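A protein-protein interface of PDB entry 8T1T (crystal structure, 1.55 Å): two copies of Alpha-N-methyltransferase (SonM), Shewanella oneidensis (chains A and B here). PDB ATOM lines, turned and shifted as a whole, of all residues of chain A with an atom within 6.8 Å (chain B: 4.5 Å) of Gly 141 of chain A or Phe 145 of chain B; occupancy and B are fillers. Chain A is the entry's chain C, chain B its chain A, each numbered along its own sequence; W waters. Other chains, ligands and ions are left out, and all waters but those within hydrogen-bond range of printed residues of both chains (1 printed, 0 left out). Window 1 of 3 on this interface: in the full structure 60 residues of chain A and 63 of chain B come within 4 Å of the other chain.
ND1 of His 155 of chain B is in hydrogen-bond range of OD2 of Asp 158 of chain A (2.8 Å).
The side-chain amide nitrogen (NE2) of Gln 149 of chain B is in hydrogen-bond range of the backbone carbonyl oxygen (O) of Asn 139 of chain A, 2.8 Å away.
The side-chain carboxylate of Asp 136 of chain A is in hydrogen-bond range of the backbone NH of Phe 99 of chain B (2.8 Å).
The side-chain amide oxygen (OE1) of Gln 143 of chain A lies close to the side-chain amide oxygen (OE1) of Gln 143 of chain B.
The backbone NH of Ser 144 of chain B is in hydrogen-bond range of the backbone carbonyl oxygen of His 142 of chain A (2.9 Å).
A ring nitrogen (ND1) of His 155 of chain B lies close to the side-chain hydroxyl (OG1) of Thr 160 of chain A.
The backbone carbonyl oxygen (O) of Asp 158 of chain A sits at hydrogen-bond distance from the side-chain hydroxyl (OG1) of Thr 161 of chain A, at 2.8 Å.
The backbone NH of Phe 145 of chain B sits at hydrogen-bond distance from the backbone carbonyl oxygen of Leu 164 of chain B, at 3.0 Å.
OE1 of Gln 149 of chain B lies within hydrogen-bond range of NE2 of His 155 of chain B.
O of Thr 160 of chain A is in hydrogen-bond range of OG of Ser 140 of chain A, at 2.7 Å.
The backbone NH (N) of Gln 143 of chain A is in hydrogen-bond range of the backbone carbonyl oxygen (O) of His 162 of chain A (3.0 Å).
The backbone carbonyl oxygen (O) of Gln 143 of chain B lies within hydrogen-bond range of the backbone NH (N) of Leu 164 of chain B (2.8 Å).
Among the printed residues, pairs that only touch across the chains: Ser 140 of chain A with His 155 of chain B (3.1 Å), His 142 of chain A with Gln 143 of chain B (3.2 Å), Gly 141 of chain A with Ser 144 of chain B (3.3 Å), Ser 140 of chain A with Gln 149 of chain B (3.4 Å), Gly 138 of chain A with Gln 149 of chain B (3.5 Å), Thr 161 of chain A with Phe 145 of chain B (3.5 Å), Leu 245 of chain A with His 155 of chain B (3.6 Å), Gly 138 of chain A with Phe 99 of chain B (3.6 Å), Leu 245 of chain A with Gln 149 of chain B (3.8 Å), Asp 158 of chain A with Phe 145 of chain B (3.8 Å), Gly 141 of chain A with Gln 149 of chain B (3.9 Å) and Gly 141 of chain A with Phe 145 of chain B (3.95 Å).
Of chain B, only Ser 144 (3.3 Å), Phe 145 (3.95 Å) and Gln 149 (3.9 Å) come within 4 Å of Gly 141 of chain A.
Printed residues of chain B within 4 Å of Thr 160 of chain A: His 155.
Leu 163 of chain A touches none of the printed residues of chain B.
Of the printed residues of chain A, Phe 99 of chain B touches Asp 136 and Gly 138.
The nearest residue of chain A that does not touch Phe 145 of chain B is Ser 140 of chain A (4.5 Å).
The nearest printed residue of chain B that does not touch Thr 160 of chain A is Phe 145 of chain B (5.6 Å).
Of the 13 printed residues of chain B, 6 touch a printed residue of chain A.
Of the 16 printed residues of chain A, 11 touch a printed residue of chain B.
Printed residues of chain A that touch a printed residue of chain B: Asp 136, Gly 138, Asn 139, Ser 140, Gly 141, His 142, Gln 143, Asp 158, Thr 160, Thr 161 and Leu 245.
Hydrophobic or aromatic side chains of chain A that line the printed part of chain B: His 142 and Leu 245.
Among the printed residues, 18 pairs touch across the chains.
Among the printed residues, no Asp or Glu carboxylate lies within 4 Å of a Lys or Arg side-chain nitrogen of the other chain.
Gln 143 of chain A touches its own counterpart, Gln 143 of chain B.
2 positions are printed for both chains.
Water W1 lies within hydrogen-bond range of the side-chain amide oxygen (OE1) of Gln 149 of chain B (2.9 Å), the backbone NH (N) of Glu 146 of chain B (2.9 Å), the backbone carbonyl oxygen (O) of Gly 138 of chain A (2.9 Å) and the backbone NH (N) of Gly 141 of chain A (3.4 Å).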
ATOM      1  N   TRP A 130     -29.087 -20.562  -4.937  1.00  0.00           N
ATOM      2  CA  TRP A 130     -28.183 -20.404  -6.065  1.00  0.00           C
ATOM      3  C   TRP A 130     -27.639 -21.761  -6.504  1.00  0.00           C
ATOM      4  O   TRP A 130     -27.563 -22.048  -7.697  1.00  0.00           O
ATOM      5  CB  TRP A 130     -27.034 -19.440  -5.742  1.00  0.00           C
ATOM      6  CG  TRP A 130     -27.454 -18.081  -5.278  1.00  0.00           C
ATOM      7  CD1 TRP A 130     -26.940 -17.391  -4.217  1.00  0.00           C
ATOM      8  CD2 TRP A 130     -28.462 -17.232  -5.858  1.00  0.00           C
ATOM      9  NE1 TRP A 130     -27.559 -16.178  -4.093  1.00  0.00           N
ATOM     10  CE2 TRP A 130     -28.497 -16.051  -5.086  1.00  0.00           C
ATOM     11  CE3 TRP A 130     -29.330 -17.344  -6.951  1.00  0.00           C
ATOM     12  CZ2 TRP A 130     -29.379 -15.010  -5.361  1.00  0.00           C
ATOM     13  CZ3 TRP A 130     -30.198 -16.310  -7.226  1.00  0.00           C
ATOM     14  CH2 TRP A 130     -30.215 -15.154  -6.445  1.00  0.00           C
ATOM     15  N   ASP A 136     -26.338 -18.053 -10.964  1.00  0.00           N
ATOM     16  CA  ASP A 136     -25.353 -17.160 -10.375  1.00  0.00           C
ATOM     17  C   ASP A 136     -25.990 -15.781 -10.216  1.00  0.00           C
ATOM     18  O   ASP A 136     -26.445 -15.195 -11.193  1.00  0.00           O
ATOM     19  CB  ASP A 136     -24.081 -17.119 -11.225  1.00  0.00           C
ATOM     20  CG  ASP A 136     -22.942 -16.308 -10.628  1.00  0.00           C
ATOM     21  OD1 ASP A 136     -23.205 -15.481  -9.738  1.00  0.00           O
ATOM     22  OD2 ASP A 136     -21.790 -16.512 -11.067  1.00  0.00           O
ATOM     23  N   PRO A 137     -26.052 -15.223  -8.986  1.00  0.00           N
ATOM     24  CA  PRO A 137     -26.620 -13.892  -8.765  1.00  0.00           C
ATOM     25  C   PRO A 137     -25.912 -12.811  -9.583  1.00  0.00           C
ATOM     26  O   PRO A 137     -26.491 -11.767  -9.870  1.00  0.00           O
ATOM     27  CB  PRO A 137     -26.421 -13.643  -7.261  1.00  0.00           C
ATOM     28  CG  PRO A 137     -25.354 -14.633  -6.849  1.00  0.00           C
ATOM     29  CD  PRO A 137     -25.568 -15.837  -7.740  1.00  0.00           C
ATOM     30  N   GLY A 138     -24.662 -13.092  -9.965  1.00  0.00           N
ATOM     31  CA  GLY A 138     -23.828 -12.145 -10.689  1.00  0.00           C
ATOM     32  C   GLY A 138     -24.171 -12.078 -12.178  1.00  0.00           C
ATOM     33  O   GLY A 138     -23.809 -11.120 -12.852  1.00  0.00           O
ATOM     34  N   ASN A 139     -24.880 -13.097 -12.674  1.00  0.00           N
ATOM     35  CA  ASN A 139     -25.179 -13.220 -14.095  1.00  0.00           C
ATOM     36  C   ASN A 139     -25.856 -11.952 -14.609  1.00  0.00           C
ATOM     37  O   ASN A 139     -25.419 -11.373 -15.600  1.00  0.00           O
ATOM     38  CB  ASN A 139     -26.045 -14.445 -14.386  1.00  0.00           C
ATOM     39  CG  ASN A 139     -26.078 -14.785 -15.859  1.00  0.00           C
ATOM     40  OD1 ASN A 139     -27.095 -14.590 -16.520  1.00  0.00           O
ATOM     41  ND2 ASN A 139     -24.960 -15.265 -16.382  1.00  0.00           N
ATOM     42  N   SER A 140     -26.938 -11.539 -13.946  1.00  0.00           N
ATOM     43  CA  SER A 140     -27.647 -10.331 -14.336  1.00  0.00           C
ATOM     44  C   SER A 140     -28.040  -9.523 -13.103  1.00  0.00           C
ATOM     45  O   SER A 140     -28.871  -8.625 -13.196  1.00  0.00           O
ATOM     46  CB  SER A 140     -28.839 -10.652 -15.203  1.00  0.00           C
ATOM     47  OG  SER A 140     -29.822 -11.389 -14.483  1.00  0.00           O
ATOM     48  N   GLY A 141     -27.411  -9.826 -11.963  1.00  0.00           N
ATOM     49  CA  GLY A 141     -27.677  -9.118 -10.719  1.00  0.00           C
ATOM     50  C   GLY A 141     -28.819  -9.766  -9.940  1.00  0.00           C
ATOM     51  O   GLY A 141     -29.482 -10.673 -10.435  1.00  0.00           O
ATOM     52  N   HIS A 142     -29.023  -9.328  -8.696  1.00  0.00           N
ATOM     53  CA  HIS A 142     -30.090  -9.894  -7.888  1.00  0.00           C
ATOM     54  C   HIS A 142     -30.559  -8.864  -6.862  1.00  0.00           C
ATOM     55  O   HIS A 142     -29.807  -7.978  -6.464  1.00  0.00           O
ATOM     56  CB  HIS A 142     -29.655 -11.244  -7.302  1.00  0.00           C
ATOM     57  CG  HIS A 142     -29.313 -11.242  -5.849  1.00  0.00           C
ATOM     58  ND1 HIS A 142     -30.279 -11.355  -4.872  1.00  0.00           N
ATOM     59  CD2 HIS A 142     -28.139 -11.207  -5.209  1.00  0.00           C
ATOM     60  CE1 HIS A 142     -29.697 -11.352  -3.681  1.00  0.00           C
ATOM     61  NE2 HIS A 142     -28.400 -11.260  -3.863  1.00  0.00           N
ATOM     62  N   GLN A 143     -31.826  -8.997  -6.463  1.00  0.00           N
ATOM     63  CA  GLN A 143     -32.458  -8.142  -5.478  1.00  0.00           C
ATOM     64  C   GLN A 143     -33.229  -9.060  -4.538  1.00  0.00           C
ATOM     65  O   GLN A 143     -33.857 -10.007  -4.998  1.00  0.00           O
ATOM     66  CB  GLN A 143     -33.379  -7.119  -6.153  1.00  0.00           C
ATOM     67  CG  GLN A 143     -32.653  -6.173  -7.106  1.00  0.00           C
ATOM     68  CD  GLN A 143     -33.528  -5.046  -7.605  1.00  0.00           C
ATOM     69  OE1 GLN A 143     -33.192  -3.868  -7.487  1.00  0.00           O
ATOM     70  NE2 GLN A 143     -34.655  -5.402  -8.193  1.00  0.00           N
ATOM     71  N   ASP A 158     -35.619  -4.138 -10.518  1.00  0.00           N
ATOM     72  CA  ASP A 158     -34.947  -4.142 -11.802  1.00  0.00           C
ATOM     73  C   ASP A 158     -35.257  -5.476 -12.476  1.00  0.00           C
ATOM     74  O   ASP A 158     -34.783  -6.519 -12.032  1.00  0.00           O
ATOM     75  CB  ASP A 158     -33.448  -3.896 -11.610  1.00  0.00           C
ATOM     76  CG  ASP A 158     -32.643  -3.930 -12.894  1.00  0.00           C
ATOM     77  OD1 ASP A 158     -33.219  -4.309 -13.942  1.00  0.00           O
ATOM     78  OD2 ASP A 158     -31.452  -3.570 -12.836  1.00  0.00           O
ATOM     79  N   THR A 160     -34.338  -7.067 -14.954  1.00  0.00           N
ATOM     80  CA  THR A 160     -33.259  -7.829 -15.559  1.00  0.00           C
ATOM     81  C   THR A 160     -32.623  -8.754 -14.523  1.00  0.00           C
ATOM     82  O   THR A 160     -31.880  -9.657 -14.896  1.00  0.00           O
ATOM     83  CB  THR A 160     -32.183  -6.932 -16.192  1.00  0.00           C
ATOM     84  OG1 THR A 160     -31.537  -6.169 -15.173  1.00  0.00           O
ATOM     85  CG2 THR A 160     -32.738  -5.995 -17.242  1.00  0.00           C
ATOM     86  N   THR A 161     -32.936  -8.534 -13.233  1.00  0.00           N
ATOM     87  CA  THR A 161     -32.284  -9.259 -12.152  1.00  0.00           C
ATOM     88  C   THR A 161     -33.093 -10.486 -11.739  1.00  0.00           C
ATOM     89  O   THR A 161     -34.233 -10.658 -12.160  1.00  0.00           O
ATOM     90  CB  THR A 161     -32.077  -8.372 -10.917  1.00  0.00           C
ATOM     91  OG1 THR A 161     -33.339  -8.111 -10.298  1.00  0.00           O
ATOM     92  CG2 THR A 161     -31.390  -7.065 -11.237  1.00  0.00           C
ATOM     93  N   HIS A 162     -32.467 -11.360 -10.938  1.00  0.00           N
ATOM     94  CA  HIS A 162     -33.215 -12.365 -10.199  1.00  0.00           C
ATOM     95  C   HIS A 162     -33.713 -11.723  -8.910  1.00  0.00           C
ATOM     96  O   HIS A 162     -32.910 -11.244  -8.110  1.00  0.00           O
ATOM     97  CB  HIS A 162     -32.366 -13.608  -9.903  1.00  0.00           C
ATOM     98  CG  HIS A 162     -32.180 -14.485 -11.096  1.00  0.00           C
ATOM     99  ND1 HIS A 162     -31.184 -14.282 -12.026  1.00  0.00           N
ATOM    100  CD2 HIS A 162     -32.855 -15.568 -11.497  1.00  0.00           C
ATOM    101  CE1 HIS A 162     -31.276 -15.213 -12.970  1.00  0.00           C
ATOM    102  NE2 HIS A 162     -32.284 -16.004 -12.666  1.00  0.00           N
ATOM    103  N   LEU A 163     -35.038 -11.745  -8.715  1.00  0.00           N
ATOM    104  CA  LEU A 163     -35.671 -11.100  -7.576  1.00  0.00           C
ATOM    105  C   LEU A 163     -36.180 -12.171  -6.613  1.00  0.00           C
ATOM    106  O   LEU A 163     -36.914 -13.072  -7.017  1.00  0.00           O
ATOM    107  CB  LEU A 163     -36.801 -10.205  -8.098  1.00  0.00           C
ATOM    108  CG  LEU A 163     -37.755  -9.618  -7.056  1.00  0.00           C
ATOM    109  CD1 LEU A 163     -37.036  -8.664  -6.117  1.00  0.00           C
ATOM    110  CD2 LEU A 163     -38.920  -8.905  -7.732  1.00  0.00           C
ATOM    111  N   PRO A 241     -35.637 -12.993 -14.308  1.00  0.00           N
ATOM    112  CA  PRO A 241     -35.720 -11.786 -15.122  1.00  0.00           C
ATOM    113  C   PRO A 241     -36.828 -11.825 -16.173  1.00  0.00           C
ATOM    114  O   PRO A 241     -37.090 -12.868 -16.775  1.00  0.00           O
ATOM    115  CB  PRO A 241     -34.357 -11.710 -15.830  1.00  0.00           C
ATOM    116  CG  PRO A 241     -33.435 -12.586 -15.005  1.00  0.00           C
ATOM    117  CD  PRO A 241     -34.318 -13.632 -14.358  1.00  0.00           C
ATOM    118  N   LEU A 245     -30.496  -8.305 -20.621  1.00  0.00           N
ATOM    119  CA  LEU A 245     -29.661  -7.125 -20.452  1.00  0.00           C
ATOM    120  C   LEU A 245     -29.587  -6.347 -21.765  1.00  0.00           C
ATOM    121  O   LEU A 245     -29.538  -6.939 -22.838  1.00  0.00           O
ATOM    122  CB  LEU A 245     -28.264  -7.578 -20.014  1.00  0.00           C
ATOM    123  CG  LEU A 245     -28.157  -8.123 -18.592  1.00  0.00           C
ATOM    124  CD1 LEU A 245     -26.752  -8.640 -18.318  1.00  0.00           C
ATOM    125  CD2 LEU A 245     -28.534  -7.059 -17.574  1.00  0.00           C
ATOM    126  N   PHE B  99     -20.918 -15.127  -8.097  1.00  0.00           N
ATOM    127  CA  PHE B  99     -19.962 -14.341  -8.864  1.00  0.00           C
ATOM    128  C   PHE B  99     -18.788 -15.234  -9.258  1.00  0.00           C
ATOM    129  O   PHE B  99     -17.627 -14.856  -9.108  1.00  0.00           O
ATOM    130  CB  PHE B  99     -19.527 -13.089  -8.092  1.00  0.00           C
ATOM    131  CG  PHE B  99     -20.560 -11.990  -8.054  1.00  0.00           C
ATOM    132  CD1 PHE B  99     -21.586 -12.009  -7.124  1.00  0.00           C
ATOM    133  CD2 PHE B  99     -20.541 -10.963  -8.988  1.00  0.00           C
ATOM    134  CE1 PHE B  99     -22.543 -11.007  -7.096  1.00  0.00           C
ATOM    135  CE2 PHE B  99     -21.501  -9.964  -8.962  1.00  0.00           C
ATOM    136  CZ  PHE B  99     -22.505  -9.990  -8.023  1.00  0.00           C
ATOM    137  N   GLN B 143     -29.312  -5.643  -2.715  1.00  0.00           N
ATOM    138  CA  GLN B 143     -29.177  -5.872  -4.141  1.00  0.00           C
ATOM    139  C   GLN B 143     -27.694  -5.902  -4.487  1.00  0.00           C
ATOM    140  O   GLN B 143     -26.917  -5.161  -3.890  1.00  0.00           O
ATOM    141  CB  GLN B 143     -29.900  -4.781  -4.930  1.00  0.00           C
ATOM    142  CG  GLN B 143     -29.320  -3.393  -4.709  1.00  0.00           C
ATOM    143  CD  GLN B 143     -30.309  -2.281  -4.969  1.00  0.00           C
ATOM    144  OE1 GLN B 143     -31.026  -2.268  -5.969  1.00  0.00           O
ATOM    145  NE2 GLN B 143     -30.344  -1.320  -4.059  1.00  0.00           N
ATOM    146  N   SER B 144     -27.332  -6.777  -5.431  1.00  0.00           N
ATOM    147  CA  SER B 144     -25.951  -6.987  -5.840  1.00  0.00           C
ATOM    148  C   SER B 144     -25.838  -6.937  -7.359  1.00  0.00           C
ATOM    149  O   SER B 144     -26.631  -7.555  -8.058  1.00  0.00           O
ATOM    150  CB  SER B 144     -25.430  -8.315  -5.335  1.00  0.00           C
ATOM    151  OG  SER B 144     -25.216  -8.292  -3.933  1.00  0.00           O
ATOM    152  N   PHE B 145     -24.798  -6.239  -7.844  1.00  0.00           N
ATOM    153  CA  PHE B 145     -24.451  -6.191  -9.254  1.00  0.00           C
ATOM    154  C   PHE B 145     -22.931  -6.219  -9.382  1.00  0.00           C
ATOM    155  O   PHE B 145     -22.227  -5.741  -8.494  1.00  0.00           O
ATOM    156  CB  PHE B 145     -24.938  -4.901  -9.925  1.00  0.00           C
ATOM    157  CG  PHE B 145     -26.410  -4.603  -9.806  1.00  0.00           C
ATOM    158  CD1 PHE B 145     -27.325  -5.181 -10.672  1.00  0.00           C
ATOM    159  CD2 PHE B 145     -26.879  -3.727  -8.838  1.00  0.00           C
ATOM    160  CE1 PHE B 145     -28.679  -4.899 -10.561  1.00  0.00           C
ATOM    161  CE2 PHE B 145     -28.233  -3.445  -8.732  1.00  0.00           C
ATOM    162  CZ  PHE B 145     -29.129  -4.034  -9.593  1.00  0.00           C
ATOM    163  N   GLU B 146     -22.440  -6.796 -10.479  1.00  0.00           N
ATOM    164  CA  GLU B 146     -21.045  -6.648 -10.853  1.00  0.00           C
ATOM    165  C   GLU B 146     -20.861  -5.209 -11.332  1.00  0.00           C
ATOM    166  O   GLU B 146     -21.668  -4.728 -12.125  1.00  0.00           O
ATOM    167  CB  GLU B 146     -20.695  -7.695 -11.912  1.00  0.00           C
ATOM    168  CG  GLU B 146     -19.213  -7.999 -12.023  1.00  0.00           C
ATOM    169  CD  GLU B 146     -18.478  -7.342 -13.178  1.00  0.00           C
ATOM    170  OE1 GLU B 146     -19.151  -6.766 -14.061  1.00  0.00           O
ATOM    171  OE2 GLU B 146     -17.229  -7.423 -13.202  1.00  0.00           O
ATOM    172  N   ALA B 147     -19.809  -4.536 -10.848  1.00  0.00           N
ATOM    173  CA  ALA B 147     -19.627  -3.110 -11.092  1.00  0.00           C
ATOM    174  C   ALA B 147     -19.601  -2.811 -12.592  1.00  0.00           C
ATOM    175  O   ALA B 147     -20.243  -1.866 -13.056  1.00  0.00           O
ATOM    176  CB  ALA B 147     -18.370  -2.625 -10.413  1.00  0.00           C
ATOM    177  N   GLN B 149     -20.795  -4.593 -15.102  1.00  0.00           N
ATOM    178  CA  GLN B 149     -22.081  -4.849 -15.723  1.00  0.00           C
ATOM    179  C   GLN B 149     -23.026  -3.674 -15.466  1.00  0.00           C
ATOM    180  O   GLN B 149     -23.850  -3.338 -16.319  1.00  0.00           O
ATOM    181  CB  GLN B 149     -22.683  -6.149 -15.198  1.00  0.00           C
ATOM    182  CG  GLN B 149     -23.941  -6.557 -15.942  1.00  0.00           C
ATOM    183  CD  GLN B 149     -24.587  -7.780 -15.342  1.00  0.00           C
ATOM    184  OE1 GLN B 149     -25.601  -7.691 -14.655  1.00  0.00           O
ATOM    185  NE2 GLN B 149     -23.991  -8.935 -15.592  1.00  0.00           N
ATOM    186  N   PHE B 150     -22.900  -3.069 -14.275  1.00  0.00           N
ATOM    187  CA  PHE B 150     -23.697  -1.913 -13.894  1.00  0.00           C
ATOM    188  C   PHE B 150     -23.402  -0.753 -14.845  1.00  0.00           C
ATOM    189  O   PHE B 150     -24.262   0.082 -15.110  1.00  0.00           O
ATOM    190  CB  PHE B 150     -23.413  -1.527 -12.438  1.00  0.00           C
ATOM    191  CG  PHE B 150     -24.345  -0.483 -11.878  1.00  0.00           C
ATOM    192  CD1 PHE B 150     -25.546  -0.846 -11.289  1.00  0.00           C
ATOM    193  CD2 PHE B 150     -24.040   0.865 -11.968  1.00  0.00           C
ATOM    194  CE1 PHE B 150     -26.407   0.114 -10.781  1.00  0.00           C
ATOM    195  CE2 PHE B 150     -24.906   1.825 -11.467  1.00  0.00           C
ATOM    196  CZ  PHE B 150     -26.087   1.448 -10.870  1.00  0.00           C
ATOM    197  N   HIS B 155     -28.994  -1.010 -15.633  1.00  0.00           N
ATOM    198  CA  HIS B 155     -29.453  -1.434 -14.320  1.00  0.00           C
ATOM    199  C   HIS B 155     -29.872  -0.207 -13.513  1.00  0.00           C
ATOM    200  O   HIS B 155     -29.188   0.815 -13.518  1.00  0.00           O
ATOM    201  CB  HIS B 155     -28.346  -2.178 -13.562  1.00  0.00           C
ATOM    202  CG  HIS B 155     -28.129  -3.599 -13.963  1.00  0.00           C
ATOM    203  ND1 HIS B 155     -29.111  -4.564 -13.891  1.00  0.00           N
ATOM    204  CD2 HIS B 155     -27.018  -4.228 -14.373  1.00  0.00           C
ATOM    205  CE1 HIS B 155     -28.605  -5.729 -14.277  1.00  0.00           C
ATOM    206  NE2 HIS B 155     -27.334  -5.548 -14.572  1.00  0.00           N
ATOM    207  N   LEU B 163     -26.908  -1.515  -1.447  1.00  0.00           N
ATOM    208  CA  LEU B 163     -26.426  -1.843  -2.781  1.00  0.00           C
ATOM    209  C   LEU B 163     -24.974  -2.312  -2.693  1.00  0.00           C
ATOM    210  O   LEU B 163     -24.122  -1.626  -2.127  1.00  0.00           O
ATOM    211  CB  LEU B 163     -26.572  -0.611  -3.683  1.00  0.00           C
ATOM    212  CG  LEU B 163     -25.830  -0.652  -5.019  1.00  0.00           C
ATOM    213  CD1 LEU B 163     -26.418  -1.709  -5.940  1.00  0.00           C
ATOM    214  CD2 LEU B 163     -25.859   0.711  -5.694  1.00  0.00           C
ATOM    215  N   LEU B 164     -24.720  -3.500  -3.248  1.00  0.00           N
ATOM    216  CA  LEU B 164     -23.384  -4.073  -3.300  1.00  0.00           C
ATOM    217  C   LEU B 164     -22.885  -4.056  -4.740  1.00  0.00           C
ATOM    218  O   LEU B 164     -23.535  -4.625  -5.616  1.00  0.00           O
ATOM    219  CB  LEU B 164     -23.436  -5.511  -2.769  1.00  0.00           C
ATOM    220  CG  LEU B 164     -23.482  -5.677  -1.252  1.00  0.00           C
ATOM    221  CD1 LEU B 164     -24.856  -5.330  -0.695  1.00  0.00           C
ATOM    222  CD2 LEU B 164     -23.096  -7.096  -0.865  1.00  0.00           C
ATOM    223  N   LEU B 165     -21.731  -3.409  -4.980  1.00  0.00           N
ATOM    224  CA  LEU B 165     -21.056  -3.510  -6.264  1.00  0.00           C
ATOM    225  C   LEU B 165     -19.813  -4.388  -6.119  1.00  0.00           C
ATOM    226  O   LEU B 165     -18.856  -4.021  -5.444  1.00  0.00           O
ATOM    227  CB  LEU B 165     -20.698  -2.109  -6.768  1.00  0.00           C
ATOM    228  CG  LEU B 165     -21.878  -1.199  -7.113  1.00  0.00           C
ATOM    229  CD1 LEU B 165     -21.391   0.108  -7.719  1.00  0.00           C
ATOM    230  CD2 LEU B 165     -22.842  -1.888  -8.065  1.00  0.00           C
ATOM    231  N   TRP B 166     -19.863  -5.569  -6.738  1.00  0.00           N
ATOM    232  CA  TRP B 166     -18.772  -6.525  -6.676  1.00  0.00           C
ATOM    233  C   TRP B 166     -17.744  -6.206  -7.760  1.00  0.00           C
ATOM    234  O   TRP B 166     -18.067  -5.595  -8.776  1.00  0.00           O
ATOM    235  CB  TRP B 166     -19.292  -7.955  -6.836  1.00  0.00           C
ATOM    236  CG  TRP B 166     -20.290  -8.415  -5.817  1.00  0.00           C
ATOM    237  CD1 TRP B 166     -21.495  -7.853  -5.509  1.00  0.00           C
ATOM    238  CD2 TRP B 166     -20.195  -9.607  -5.020  1.00  0.00           C
ATOM    239  NE1 TRP B 166     -22.146  -8.599  -4.563  1.00  0.00           N
ATOM    240  CE2 TRP B 166     -21.374  -9.686  -4.248  1.00  0.00           C
ATOM    241  CE3 TRP B 166     -19.230 -10.614  -4.881  1.00  0.00           C
ATOM    242  CZ2 TRP B 166     -21.607 -10.725  -3.347  1.00  0.00           C
ATOM    243  CZ3 TRP B 166     -19.465 -11.641  -3.995  1.00  0.00           C
ATOM    244  CH2 TRP B 166     -20.634 -11.692  -3.236  1.00  0.00           C
HETATM  245  O   HOH W   1     -24.363  -8.330 -12.089  1.00  0.00           O
